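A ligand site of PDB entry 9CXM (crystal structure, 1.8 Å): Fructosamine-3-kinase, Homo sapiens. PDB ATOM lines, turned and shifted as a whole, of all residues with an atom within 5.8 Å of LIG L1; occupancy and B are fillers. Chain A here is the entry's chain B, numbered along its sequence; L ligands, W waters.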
ATOM      1  N   GLY A  19      -5.637  -2.217  14.301  1.00  0.00           N
ATOM      2  CA  GLY A  19      -4.403  -2.481  13.582  1.00  0.00           C
ATOM      3  C   GLY A  19      -4.703  -2.892  12.158  1.00  0.00           C
ATOM      4  O   GLY A  19      -3.804  -3.310  11.415  1.00  0.00           O
ATOM      5  N   ALA A  23       3.464  -4.414   9.008  1.00  0.00           N
ATOM      6  CA  ALA A  23       2.125  -5.016   8.877  1.00  0.00           C
ATOM      7  C   ALA A  23       1.930  -5.558   7.465  1.00  0.00           C
ATOM      8  O   ALA A  23       2.451  -4.965   6.516  1.00  0.00           O
ATOM      9  CB  ALA A  23       1.043  -3.999   9.214  1.00  0.00           C
ATOM     10  N   GLY A  24       1.162  -6.648   7.317  1.00  0.00           N
ATOM     11  CA  GLY A  24       0.872  -7.375   6.087  1.00  0.00           C
ATOM     12  C   GLY A  24       1.564  -8.746   6.057  1.00  0.00           C
ATOM     13  O   GLY A  24       2.600  -8.951   6.709  1.00  0.00           O
ATOM     14  N   CYS A  25       1.002  -9.682   5.276  1.00  0.00           N
ATOM     15  CA  CYS A  25       1.618 -11.018   5.196  1.00  0.00           C
ATOM     16  C   CYS A  25       2.560 -11.185   4.018  1.00  0.00           C
ATOM     17  O   CYS A  25       3.180 -12.240   3.874  1.00  0.00           O
ATOM     18  CB  CYS A  25       0.570 -12.150   5.135  1.00  0.00           C
ATOM     19  SG  CYS A  25      -0.648 -12.288   6.429  1.00  0.00           S
ATOM     20  N   ILE A  26       2.682 -10.176   3.171  1.00  0.00           N
ATOM     21  CA  ILE A  26       3.469 -10.257   1.957  1.00  0.00           C
ATOM     22  C   ILE A  26       4.661  -9.337   2.030  1.00  0.00           C
ATOM     23  O   ILE A  26       5.796  -9.740   1.752  1.00  0.00           O
ATOM     24  CB  ILE A  26       2.586  -9.940   0.718  1.00  0.00           C
ATOM     25  CG1 ILE A  26       1.453 -10.975   0.544  1.00  0.00           C
ATOM     26  CG2 ILE A  26       3.420  -9.857  -0.551  1.00  0.00           C
ATOM     27  CD1 ILE A  26       2.035 -12.420   0.348  1.00  0.00           C
ATOM     28  N   SER A  27       4.434  -8.084   2.427  1.00  0.00           N
ATOM     29  CA  SER A  27       5.472  -7.066   2.431  1.00  0.00           C
ATOM     30  C   SER A  27       5.553  -6.462   3.829  1.00  0.00           C
ATOM     31  O   SER A  27       4.635  -6.603   4.641  1.00  0.00           O
ATOM     32  CB  SER A  27       5.145  -5.948   1.425  1.00  0.00           C
ATOM     33  OG  SER A  27       4.978  -6.472   0.107  1.00  0.00           O
ATOM     34  N   GLU A  28       6.634  -5.748   4.076  1.00  0.00           N
ATOM     35  CA  GLU A  28       6.773  -4.972   5.306  1.00  0.00           C
ATOM     36  C   GLU A  28       6.206  -3.574   5.025  1.00  0.00           C
ATOM     37  O   GLU A  28       6.625  -2.939   4.061  1.00  0.00           O
ATOM     38  CB  GLU A  28       8.246  -4.907   5.688  1.00  0.00           C
ATOM     39  CG  GLU A  28       8.558  -4.054   6.893  1.00  0.00           C
ATOM     40  CD  GLU A  28       9.997  -4.219   7.322  1.00  0.00           C
ATOM     41  OE1 GLU A  28      10.741  -4.973   6.639  1.00  0.00           O
ATOM     42  OE2 GLU A  28      10.385  -3.598   8.345  1.00  0.00           O
ATOM     43  N   GLY A  29       5.210  -3.145   5.797  1.00  0.00           N
ATOM     44  CA  GLY A  29       4.534  -1.858   5.616  1.00  0.00           C
ATOM     45  C   GLY A  29       4.804  -0.857   6.729  1.00  0.00           C
ATOM     46  O   GLY A  29       4.696  -1.202   7.907  1.00  0.00           O
ATOM     47  N   ALA A  31       4.462   3.584   7.813  1.00  0.00           N
ATOM     48  CA  ALA A  31       4.048   4.957   7.518  1.00  0.00           C
ATOM     49  C   ALA A  31       5.124   5.958   7.950  1.00  0.00           C
ATOM     50  O   ALA A  31       5.736   5.808   9.017  1.00  0.00           O
ATOM     51  CB  ALA A  31       2.762   5.315   8.229  1.00  0.00           C
ATOM     52  N   PHE A  40       2.770   5.891   2.856  1.00  0.00           N
ATOM     53  CA  PHE A  40       2.839   4.513   3.307  1.00  0.00           C
ATOM     54  C   PHE A  40       3.752   3.767   2.369  1.00  0.00           C
ATOM     55  O   PHE A  40       3.673   3.949   1.164  1.00  0.00           O
ATOM     56  CB  PHE A  40       1.431   3.874   3.341  1.00  0.00           C
ATOM     57  CG  PHE A  40       1.433   2.536   3.932  1.00  0.00           C
ATOM     58  CD1 PHE A  40       1.551   2.390   5.300  1.00  0.00           C
ATOM     59  CD2 PHE A  40       1.316   1.402   3.127  1.00  0.00           C
ATOM     60  CE1 PHE A  40       1.584   1.130   5.871  1.00  0.00           C
ATOM     61  CE2 PHE A  40       1.339   0.120   3.702  1.00  0.00           C
ATOM     62  CZ  PHE A  40       1.478   0.017   5.087  1.00  0.00           C
ATOM     63  N   LYS A  42       5.575   0.057   1.324  1.00  0.00           N
ATOM     64  CA  LYS A  42       5.721  -1.414   1.357  1.00  0.00           C
ATOM     65  C   LYS A  42       7.081  -1.815   0.821  1.00  0.00           C
ATOM     66  O   LYS A  42       7.545  -1.312  -0.194  1.00  0.00           O
ATOM     67  CB  LYS A  42       4.638  -2.111   0.486  1.00  0.00           C
ATOM     68  CG  LYS A  42       3.290  -1.961   1.221  1.00  0.00           C
ATOM     69  CD  LYS A  42       2.250  -3.051   0.891  1.00  0.00           C
ATOM     70  CE  LYS A  42       1.547  -2.767  -0.372  1.00  0.00           C
ATOM     71  NZ  LYS A  42       0.481  -3.849  -0.668  1.00  0.00           N
ATOM     72  N   GLU A  56       0.396  -3.935  -8.688  1.00  0.00           N
ATOM     73  CA  GLU A  56      -0.459  -3.255  -7.725  1.00  0.00           C
ATOM     74  C   GLU A  56      -0.697  -1.843  -8.202  1.00  0.00           C
ATOM     75  O   GLU A  56      -1.808  -1.311  -8.084  1.00  0.00           O
ATOM     76  CB  GLU A  56       0.217  -3.294  -6.318  1.00  0.00           C
ATOM     77  CG  GLU A  56      -0.711  -2.778  -5.227  1.00  0.00           C
ATOM     78  CD  GLU A  56      -0.121  -2.922  -3.836  1.00  0.00           C
ATOM     79  OE1 GLU A  56       0.893  -3.629  -3.694  1.00  0.00           O
ATOM     80  OE2 GLU A  56      -0.695  -2.383  -2.889  1.00  0.00           O
ATOM     81  N   PRO A  72      -5.651   4.130  -2.298  1.00  0.00           N
ATOM     82  CA  PRO A  72      -4.477   5.012  -2.209  1.00  0.00           C
ATOM     83  C   PRO A  72      -3.882   5.320  -3.571  1.00  0.00           C
ATOM     84  O   PRO A  72      -3.823   4.469  -4.464  1.00  0.00           O
ATOM     85  CB  PRO A  72      -3.469   4.193  -1.380  1.00  0.00           C
ATOM     86  CG  PRO A  72      -4.228   3.048  -0.794  1.00  0.00           C
ATOM     87  CD  PRO A  72      -5.434   2.826  -1.638  1.00  0.00           C
ATOM     88  N   MET A  89       3.145   4.941  -1.490  1.00  0.00           N
ATOM     89  CA  MET A  89       1.778   5.323  -1.915  1.00  0.00           C
ATOM     90  C   MET A  89       1.202   6.338  -0.932  1.00  0.00           C
ATOM     91  O   MET A  89       1.801   6.534   0.139  1.00  0.00           O
ATOM     92  CB  MET A  89       0.861   4.099  -1.968  1.00  0.00           C
ATOM     93  CG  MET A  89       0.428   3.611  -0.593  1.00  0.00           C
ATOM     94  SD  MET A  89      -0.437   2.026  -0.692  1.00  0.00           S
ATOM     95  CE  MET A  89       0.943   0.908  -0.917  1.00  0.00           C
ATOM     96  N   GLU A  90       0.072   6.938  -1.290  1.00  0.00           N
ATOM     97  CA  GLU A  90      -0.612   7.918  -0.402  1.00  0.00           C
ATOM     98  C   GLU A  90      -0.935   7.242   0.926  1.00  0.00           C
ATOM     99  O   GLU A  90      -1.426   6.101   0.908  1.00  0.00           O
ATOM    100  CB  GLU A  90      -1.886   8.394  -1.093  1.00  0.00           C
ATOM    101  CG  GLU A  90      -2.830   9.193  -0.221  1.00  0.00           C
ATOM    102  CD  GLU A  90      -4.172   9.409  -0.890  1.00  0.00           C
ATOM    103  OE1 GLU A  90      -4.456   8.710  -1.887  1.00  0.00           O
ATOM    104  OE2 GLU A  90      -4.924  10.287  -0.432  1.00  0.00           O
ATOM    105  N   HIS A  91      -0.663   7.922   2.045  1.00  0.00           N
ATOM    106  CA  HIS A  91      -1.042   7.371   3.370  1.00  0.00           C
ATOM    107  C   HIS A  91      -2.509   7.689   3.638  1.00  0.00           C
ATOM    108  O   HIS A  91      -2.914   8.838   3.380  1.00  0.00           O
ATOM    109  CB  HIS A  91      -0.145   7.916   4.485  1.00  0.00           C
ATOM    110  CG  HIS A  91      -0.542   7.436   5.838  1.00  0.00           C
ATOM    111  ND1 HIS A  91      -1.523   8.045   6.587  1.00  0.00           N
ATOM    112  CD2 HIS A  91      -0.095   6.397   6.584  1.00  0.00           C
ATOM    113  CE1 HIS A  91      -1.662   7.415   7.729  1.00  0.00           C
ATOM    114  NE2 HIS A  91      -0.801   6.393   7.748  1.00  0.00           N
ATOM    115  N   LEU A  92      -3.263   6.713   4.147  1.00  0.00           N
ATOM    116  CA  LEU A  92      -4.706   6.941   4.422  1.00  0.00           C
ATOM    117  C   LEU A  92      -5.025   6.587   5.875  1.00  0.00           C
ATOM    118  O   LEU A  92      -4.749   5.440   6.281  1.00  0.00           O
ATOM    119  CB  LEU A  92      -5.544   6.074   3.462  1.00  0.00           C
ATOM    120  CG  LEU A  92      -5.398   6.427   1.984  1.00  0.00           C
ATOM    121  CD1 LEU A  92      -6.229   5.476   1.127  1.00  0.00           C
ATOM    122  CD2 LEU A  92      -5.808   7.868   1.728  1.00  0.00           C
ATOM    123  N   LYS A  93      -5.531   7.548   6.632  1.00  0.00           N
ATOM    124  CA  LYS A  93      -5.972   7.271   8.002  1.00  0.00           C
ATOM    125  C   LYS A  93      -7.218   6.375   7.956  1.00  0.00           C
ATOM    126  O   LYS A  93      -8.212   6.731   7.319  1.00  0.00           O
ATOM    127  CB  LYS A  93      -6.301   8.569   8.743  1.00  0.00           C
ATOM    128  CG  LYS A  93      -5.153   9.479   8.961  1.00  0.00           C
ATOM    129  CD  LYS A  93      -5.620  10.736   9.759  1.00  0.00           C
ATOM    130  CE  LYS A  93      -6.304  11.718   8.828  1.00  0.00           C
ATOM    131  NZ  LYS A  93      -5.547  11.981   7.536  1.00  0.00           N
ATOM    132  N   MET A  94      -7.139   5.223   8.594  1.00  0.00           N
ATOM    133  CA  MET A  94      -8.093   4.140   8.429  1.00  0.00           C
ATOM    134  C   MET A  94      -8.374   3.414   9.724  1.00  0.00           C
ATOM    135  O   MET A  94      -7.475   3.245  10.551  1.00  0.00           O
ATOM    136  CB  MET A  94      -7.527   3.115   7.417  1.00  0.00           C
ATOM    137  CG  MET A  94      -7.567   3.641   6.066  1.00  0.00           C
ATOM    138  SD  MET A  94      -6.927   2.484   4.843  1.00  0.00           S
ATOM    139  CE  MET A  94      -6.037   1.349   5.896  1.00  0.00           C
ATOM    140  N   ASP A 199      -8.597  -9.084  -4.515  1.00  0.00           N
ATOM    141  CA  ASP A 199      -8.089  -9.610  -3.223  1.00  0.00           C
ATOM    142  C   ASP A 199      -8.863  -8.975  -2.073  1.00  0.00           C
ATOM    143  O   ASP A 199      -8.291  -8.459  -1.101  1.00  0.00           O
ATOM    144  CB  ASP A 199      -6.581  -9.355  -3.126  1.00  0.00           C
ATOM    145  CG  ASP A 199      -5.919 -10.143  -1.959  1.00  0.00           C
ATOM    146  OD1 ASP A 199      -6.462 -11.167  -1.530  1.00  0.00           O
ATOM    147  OD2 ASP A 199      -4.856  -9.689  -1.503  1.00  0.00           O
ATOM    148  N   TRP A 201     -10.220  -9.475   0.751  1.00  0.00           N
ATOM    149  CA  TRP A 201     -10.435 -10.036   2.074  1.00  0.00           C
ATOM    150  C   TRP A 201     -10.589  -8.907   3.073  1.00  0.00           C
ATOM    151  O   TRP A 201     -10.273  -7.753   2.792  1.00  0.00           O
ATOM    152  CB  TRP A 201      -9.316 -11.002   2.458  1.00  0.00           C
ATOM    153  CG  TRP A 201      -8.031 -10.476   2.874  1.00  0.00           C
ATOM    154  CD1 TRP A 201      -7.083  -9.885   2.076  1.00  0.00           C
ATOM    155  CD2 TRP A 201      -7.435 -10.562   4.226  1.00  0.00           C
ATOM    156  NE1 TRP A 201      -5.929  -9.556   2.855  1.00  0.00           N
ATOM    157  CE2 TRP A 201      -6.151  -9.941   4.159  1.00  0.00           C
ATOM    158  CE3 TRP A 201      -7.862 -11.075   5.460  1.00  0.00           C
ATOM    159  CZ2 TRP A 201      -5.261  -9.838   5.289  1.00  0.00           C
ATOM    160  CZ3 TRP A 201      -6.992 -10.997   6.549  1.00  0.00           C
ATOM    161  CH2 TRP A 201      -5.704 -10.388   6.453  1.00  0.00           C
ATOM    162  N   GLY A 203      -9.064  -7.946   5.592  1.00  0.00           N
ATOM    163  CA  GLY A 203      -7.844  -7.210   5.879  1.00  0.00           C
ATOM    164  C   GLY A 203      -7.447  -6.167   4.830  1.00  0.00           C
ATOM    165  O   GLY A 203      -6.504  -5.405   5.051  1.00  0.00           O
ATOM    166  N   ASN A 204      -8.128  -6.141   3.684  1.00  0.00           N
ATOM    167  CA  ASN A 204      -7.810  -5.203   2.606  1.00  0.00           C
ATOM    168  C   ASN A 204      -8.913  -4.181   2.437  1.00  0.00           C
ATOM    169  O   ASN A 204      -8.916  -3.425   1.423  1.00  0.00           O
ATOM    170  CB  ASN A 204      -7.557  -5.939   1.253  1.00  0.00           C
ATOM    171  CG  ASN A 204      -6.176  -6.555   1.191  1.00  0.00           C
ATOM    172  OD1 ASN A 204      -5.289  -6.204   2.014  1.00  0.00           O
ATOM    173  ND2 ASN A 204      -5.937  -7.468   0.196  1.00  0.00           N
ATOM    174  N   TYR A 215      -7.752  -1.419  -0.622  1.00  0.00           N
ATOM    175  CA  TYR A 215      -6.341  -1.261  -0.978  1.00  0.00           C
ATOM    176  C   TYR A 215      -5.781  -2.644  -1.212  1.00  0.00           C
ATOM    177  O   TYR A 215      -6.488  -3.640  -1.045  1.00  0.00           O
ATOM    178  CB  TYR A 215      -5.540  -0.511   0.135  1.00  0.00           C
ATOM    179  CG  TYR A 215      -5.789  -1.087   1.545  1.00  0.00           C
ATOM    180  CD1 TYR A 215      -5.059  -2.163   2.025  1.00  0.00           C
ATOM    181  CD2 TYR A 215      -6.751  -0.518   2.353  1.00  0.00           C
ATOM    182  CE1 TYR A 215      -5.325  -2.716   3.314  1.00  0.00           C
ATOM    183  CE2 TYR A 215      -7.042  -1.026   3.602  1.00  0.00           C
ATOM    184  CZ  TYR A 215      -6.300  -2.126   4.074  1.00  0.00           C
ATOM    185  OH  TYR A 215      -6.605  -2.627   5.308  1.00  0.00           O
ATOM    186  N   ASP A 216      -4.492  -2.691  -1.623  1.00  0.00           N
ATOM    187  CA  ASP A 216      -3.789  -3.939  -1.940  1.00  0.00           C
ATOM    188  C   ASP A 216      -4.527  -4.763  -3.025  1.00  0.00           C
ATOM    189  O   ASP A 216      -4.658  -5.996  -2.860  1.00  0.00           O
ATOM    190  CB  ASP A 216      -3.699  -4.771  -0.670  1.00  0.00           C
ATOM    191  CG  ASP A 216      -2.636  -5.904  -0.748  1.00  0.00           C
ATOM    192  OD1 ASP A 216      -1.728  -5.830  -1.611  1.00  0.00           O
ATOM    193  OD2 ASP A 216      -2.718  -6.819   0.092  1.00  0.00           O
HETATM  194  P1  LIG L   1      -1.731  -8.882   2.693  1.00  0.00           P
HETATM  195  O1  LIG L   1      -1.489 -10.029   3.632  1.00  0.00           O
HETATM  196  O2  LIG L   1      -1.473  -9.189   1.165  1.00  0.00           O
HETATM  197  O3  LIG L   1      -3.126  -8.271   2.771  1.00  0.00           O
HETATM  198  P2  LIG L   1       0.434  -6.808   2.341  1.00  0.00           P
HETATM  199  O4  LIG L   1       0.372  -6.951   0.830  1.00  0.00           O
HETATM  200  O5  LIG L   1       1.825  -7.162   2.889  1.00  0.00           O
HETATM  201  O6  LIG L   1      -0.687  -7.659   3.044  1.00  0.00           O
HETATM  202  P3  LIG L   1      -1.272  -4.406   2.726  1.00  0.00           P
HETATM  203  O7  LIG L   1      -1.249  -3.543   1.506  1.00  0.00           O
HETATM  204  O8  LIG L   1      -2.482  -5.252   3.015  1.00  0.00           O
HETATM  205  O9  LIG L   1       0.041  -5.319   2.809  1.00  0.00           O
HETATM  206  O10 LIG L   1      -1.031  -3.452   3.969  1.00  0.00           O
HETATM  207  C1  LIG L   1      -0.871  -3.987   5.311  1.00  0.00           C
HETATM  208  C2  LIG L   1      -1.543  -3.052   6.287  1.00  0.00           C
HETATM  209  O11 LIG L   1      -0.970  -1.726   6.173  1.00  0.00           O
HETATM  210  C3  LIG L   1      -3.034  -2.863   6.077  1.00  0.00           C
HETATM  211  O12 LIG L   1      -3.840  -3.847   6.719  1.00  0.00           O
HETATM  212  C4  LIG L   1      -3.278  -1.479   6.691  1.00  0.00           C
HETATM  213  O13 LIG L   1      -3.406  -1.612   8.106  1.00  0.00           O
HETATM  214  C5  LIG L   1      -1.962  -0.745   6.366  1.00  0.00           C
HETATM  215  N1  LIG L   1      -2.017   0.064   5.155  1.00  0.00           N
HETATM  216  C6  LIG L   1      -1.989  -0.394   3.864  1.00  0.00           C
HETATM  217  N2  LIG L   1      -2.021   0.549   2.947  1.00  0.00           N
HETATM  218  C7  LIG L   1      -2.058   1.716   3.702  1.00  0.00           C
HETATM  219  C8  LIG L   1      -2.071   3.068   3.321  1.00  0.00           C
HETATM  220  N3  LIG L   1      -2.066   3.474   2.054  1.00  0.00           N
HETATM  221  N4  LIG L   1      -2.101   4.000   4.312  1.00  0.00           N
HETATM  222  C9  LIG L   1      -2.078   3.584   5.594  1.00  0.00           C
HETATM  223  N5  LIG L   1      -2.069   2.335   6.064  1.00  0.00           N
HETATM  224  C10 LIG L   1      -2.043   1.438   5.061  1.00  0.00           C
HETATM  225  N1  LG2 L   2      -4.605 -13.528   3.779  1.00  0.00           N
HETATM  226  C1  LG2 L   2      -4.605 -13.007   2.378  1.00  0.00           C
HETATM  227  C2  LG2 L   2      -3.255 -12.461   1.750  1.00  0.00           C
HETATM  228  O1  LG2 L   2      -2.134 -12.523   2.273  1.00  0.00           O
HETATM  229  C3  LG2 L   2      -5.955 -13.985   4.132  1.00  0.00           C
HETATM  230  C4  LG2 L   2      -5.996 -14.927   5.346  1.00  0.00           C
HETATM  231  C5  LG2 L   2      -3.575 -14.856   5.663  1.00  0.00           C
HETATM  232  C6  LG2 L   2      -3.507 -14.394   4.195  1.00  0.00           C
HETATM  233  C7  LG2 L   2      -3.368 -11.866   0.327  1.00  0.00           C
HETATM  234  C8  LG2 L   2      -2.053 -12.021  -0.498  1.00  0.00           C
HETATM  235  C9  LG2 L   2      -1.712 -13.468  -0.987  1.00  0.00           C
HETATM  236  C10 LG2 L   2      -1.386 -14.409   0.131  1.00  0.00           C
HETATM  237  O2  LG2 L   2      -4.859 -14.657   6.238  1.00  0.00           O
HETATM  238  O3  LG2 L   2      -2.618 -14.662   0.792  1.00  0.00           O
HETATM  239  O4  LG2 L   2      -2.830 -13.965  -1.757  1.00  0.00           O
HETATM  240  O5  LG2 L   2      -2.146 -11.283  -1.717  1.00  0.00           O
HETATM  241  O6  LG2 L   2      -3.667 -10.512   0.594  1.00  0.00           O
HETATM  242  O   HOH W   1      -0.946  -8.894  -1.924  1.00  0.00           O
HETATM  243  O   HOH W   2       2.625  -4.572   4.069  1.00  0.00           O
HETATM  244  O   HOH W   3      -1.834  -0.984   0.610  1.00  0.00           O
HETATM  245  O   HOH W   4      -3.826  -6.215   5.035  1.00  0.00           O
HETATM  246  O   HOH W   5       2.380  -6.622  -0.762  1.00  0.00           O
HETATM  247  O   HOH W   6      -2.014   2.125   8.806  1.00  0.00           O
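O of Gly 19 touches O13 of LIG L1, at 3.7 Å. Ala 23 touches LIG L1. Gly 24 touches LIG L1. Phe 40 touches LIG L1. Pro 72 touches LIG L1. CD2 of His 91 touches C9 of LIG L1, at 3.6 Å. O of Gly 203 touches O12 of LIG L1 (3.5 Å). 18 residues have an atom within 4 Å of LIG L1: Gly 19, Ala 23, Gly 24, Cys 25, Ile 26, Ser 27, Phe 40, Lys 42, Pro 72, Met 89, Glu 90, His 91, Leu 92, Trp 201, Gly 203, Asn 204, Tyr 215 and Asp 216. The nearest printed residue that does not touch LIG L1 is Met 94 (4.03 Å).
An oxygen (O6) of LG2 L2 lies within hydrogen-bond range of an oxygen (O2) of LIG L1 (2.6 Å).
The side-chain amino group (NZ) of Lys 42 is in salt-bridge range of an oxygen (O7) of LIG L1. N of Ser 27 is in hydrogen-bond range of O5 of LIG L1. An oxygen (O2) of LIG L1 lies close to the side-chain carboxylate of Asp 216 (2.9 Å). N3 of LIG L1 lies within hydrogen-bond range of O of Glu 90, 2.9 Å away. A nitrogen (N4) of LIG L1 sits at hydrogen-bond distance from the backbone NH (N) of Leu 92. An oxygen (O1) of LIG L1 lies within hydrogen-bond range of the backbone NH of Cys 25, 3.0 Å away. The side-chain sulfur (SG) of Cys 25 sits close to an oxygen (O1) of LIG L1 (3.7 Å). NE1 of Trp 201 sits at hydrogen-bond distance from O3 of LIG L1 (3.1 Å). O3 of LIG L1 sits close to OD1 of Asn 204, at 3.1 Å. An oxygen (O5) of LIG L1 lies within hydrogen-bond range of the backbone NH of Ile 26, 3.1 Å away. OH of Tyr 215 lies within hydrogen-bond range of O12 of LIG L1 (3.3 Å). The side-chain sulfur (SD) of Met 89 lies within hydrogen-bond range of a nitrogen (N3) of LIG L1 (3.5 Å). The indole nitrogen (NE1) of Trp 201 sits at hydrogen-bond distance from an oxygen (O6) of LG2 L2 (3.3 Å). The side-chain carboxylate (OD2) of Asp 199 lies within hydrogen-bond range of an oxygen (O6) of LG2 L2 (2.5 Å).
The side-chain amino group of Lys 42 lies within salt-bridge range of the side-chain carboxylate of Asp 216 (3.1 Å). The side-chain carboxylate of Glu 56 is in salt-bridge range of the side-chain amino group of Lys 42. OD2 of Asp 216 lies close to OD1 of Asn 204. NE1 of Trp 201 lies close to ND2 of Asn 204 (3.4 Å). N of Tyr 215 sits at hydrogen-bond distance from O of Asn 204, 3.1 Å away. The side-chain amide nitrogen (ND2) of Asn 204 lies within hydrogen-bond range of the backbone carbonyl oxygen (O) of Asp 199 (2.9 Å). The backbone carbonyl oxygen (O) of Gly 203 sits at hydrogen-bond distance from the side-chain hydroxyl (OH) of Tyr 215 (2.8 Å). The backbone carbonyl oxygen (O) of Ala 23 is in hydrogen-bond range of the backbone NH (N) of Gly 29, at 3.4 Å.
Water W5 lies within hydrogen-bond range of O4 of LIG L1 (2.6 Å), OG of Ser 27 (2.7 Å) and NZ of Lys 42 (3.4 Å). Water W4 lies within hydrogen-bond range of O8 of LIG L1, O of Gly 203 and OD1 of Asn 204. Water W3 bridges O7 of LIG L1 (2.8 Å) and SD of Met 89 (3.6 Å). Water W2 lies within hydrogen-bond range of the backbone carbonyl oxygen (O) of Ala 23, the backbone carbonyl oxygen (O) of Ser 27, an oxygen (O5) of LIG L1 and the backbone NH (N) of Gly 29. Water W1 lies within hydrogen-bond range of O5 of LG2 L2 (2.7 Å), O2 of LIG L1 (3.1 Å) and OD1 of Asp 216 (3.2 Å).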
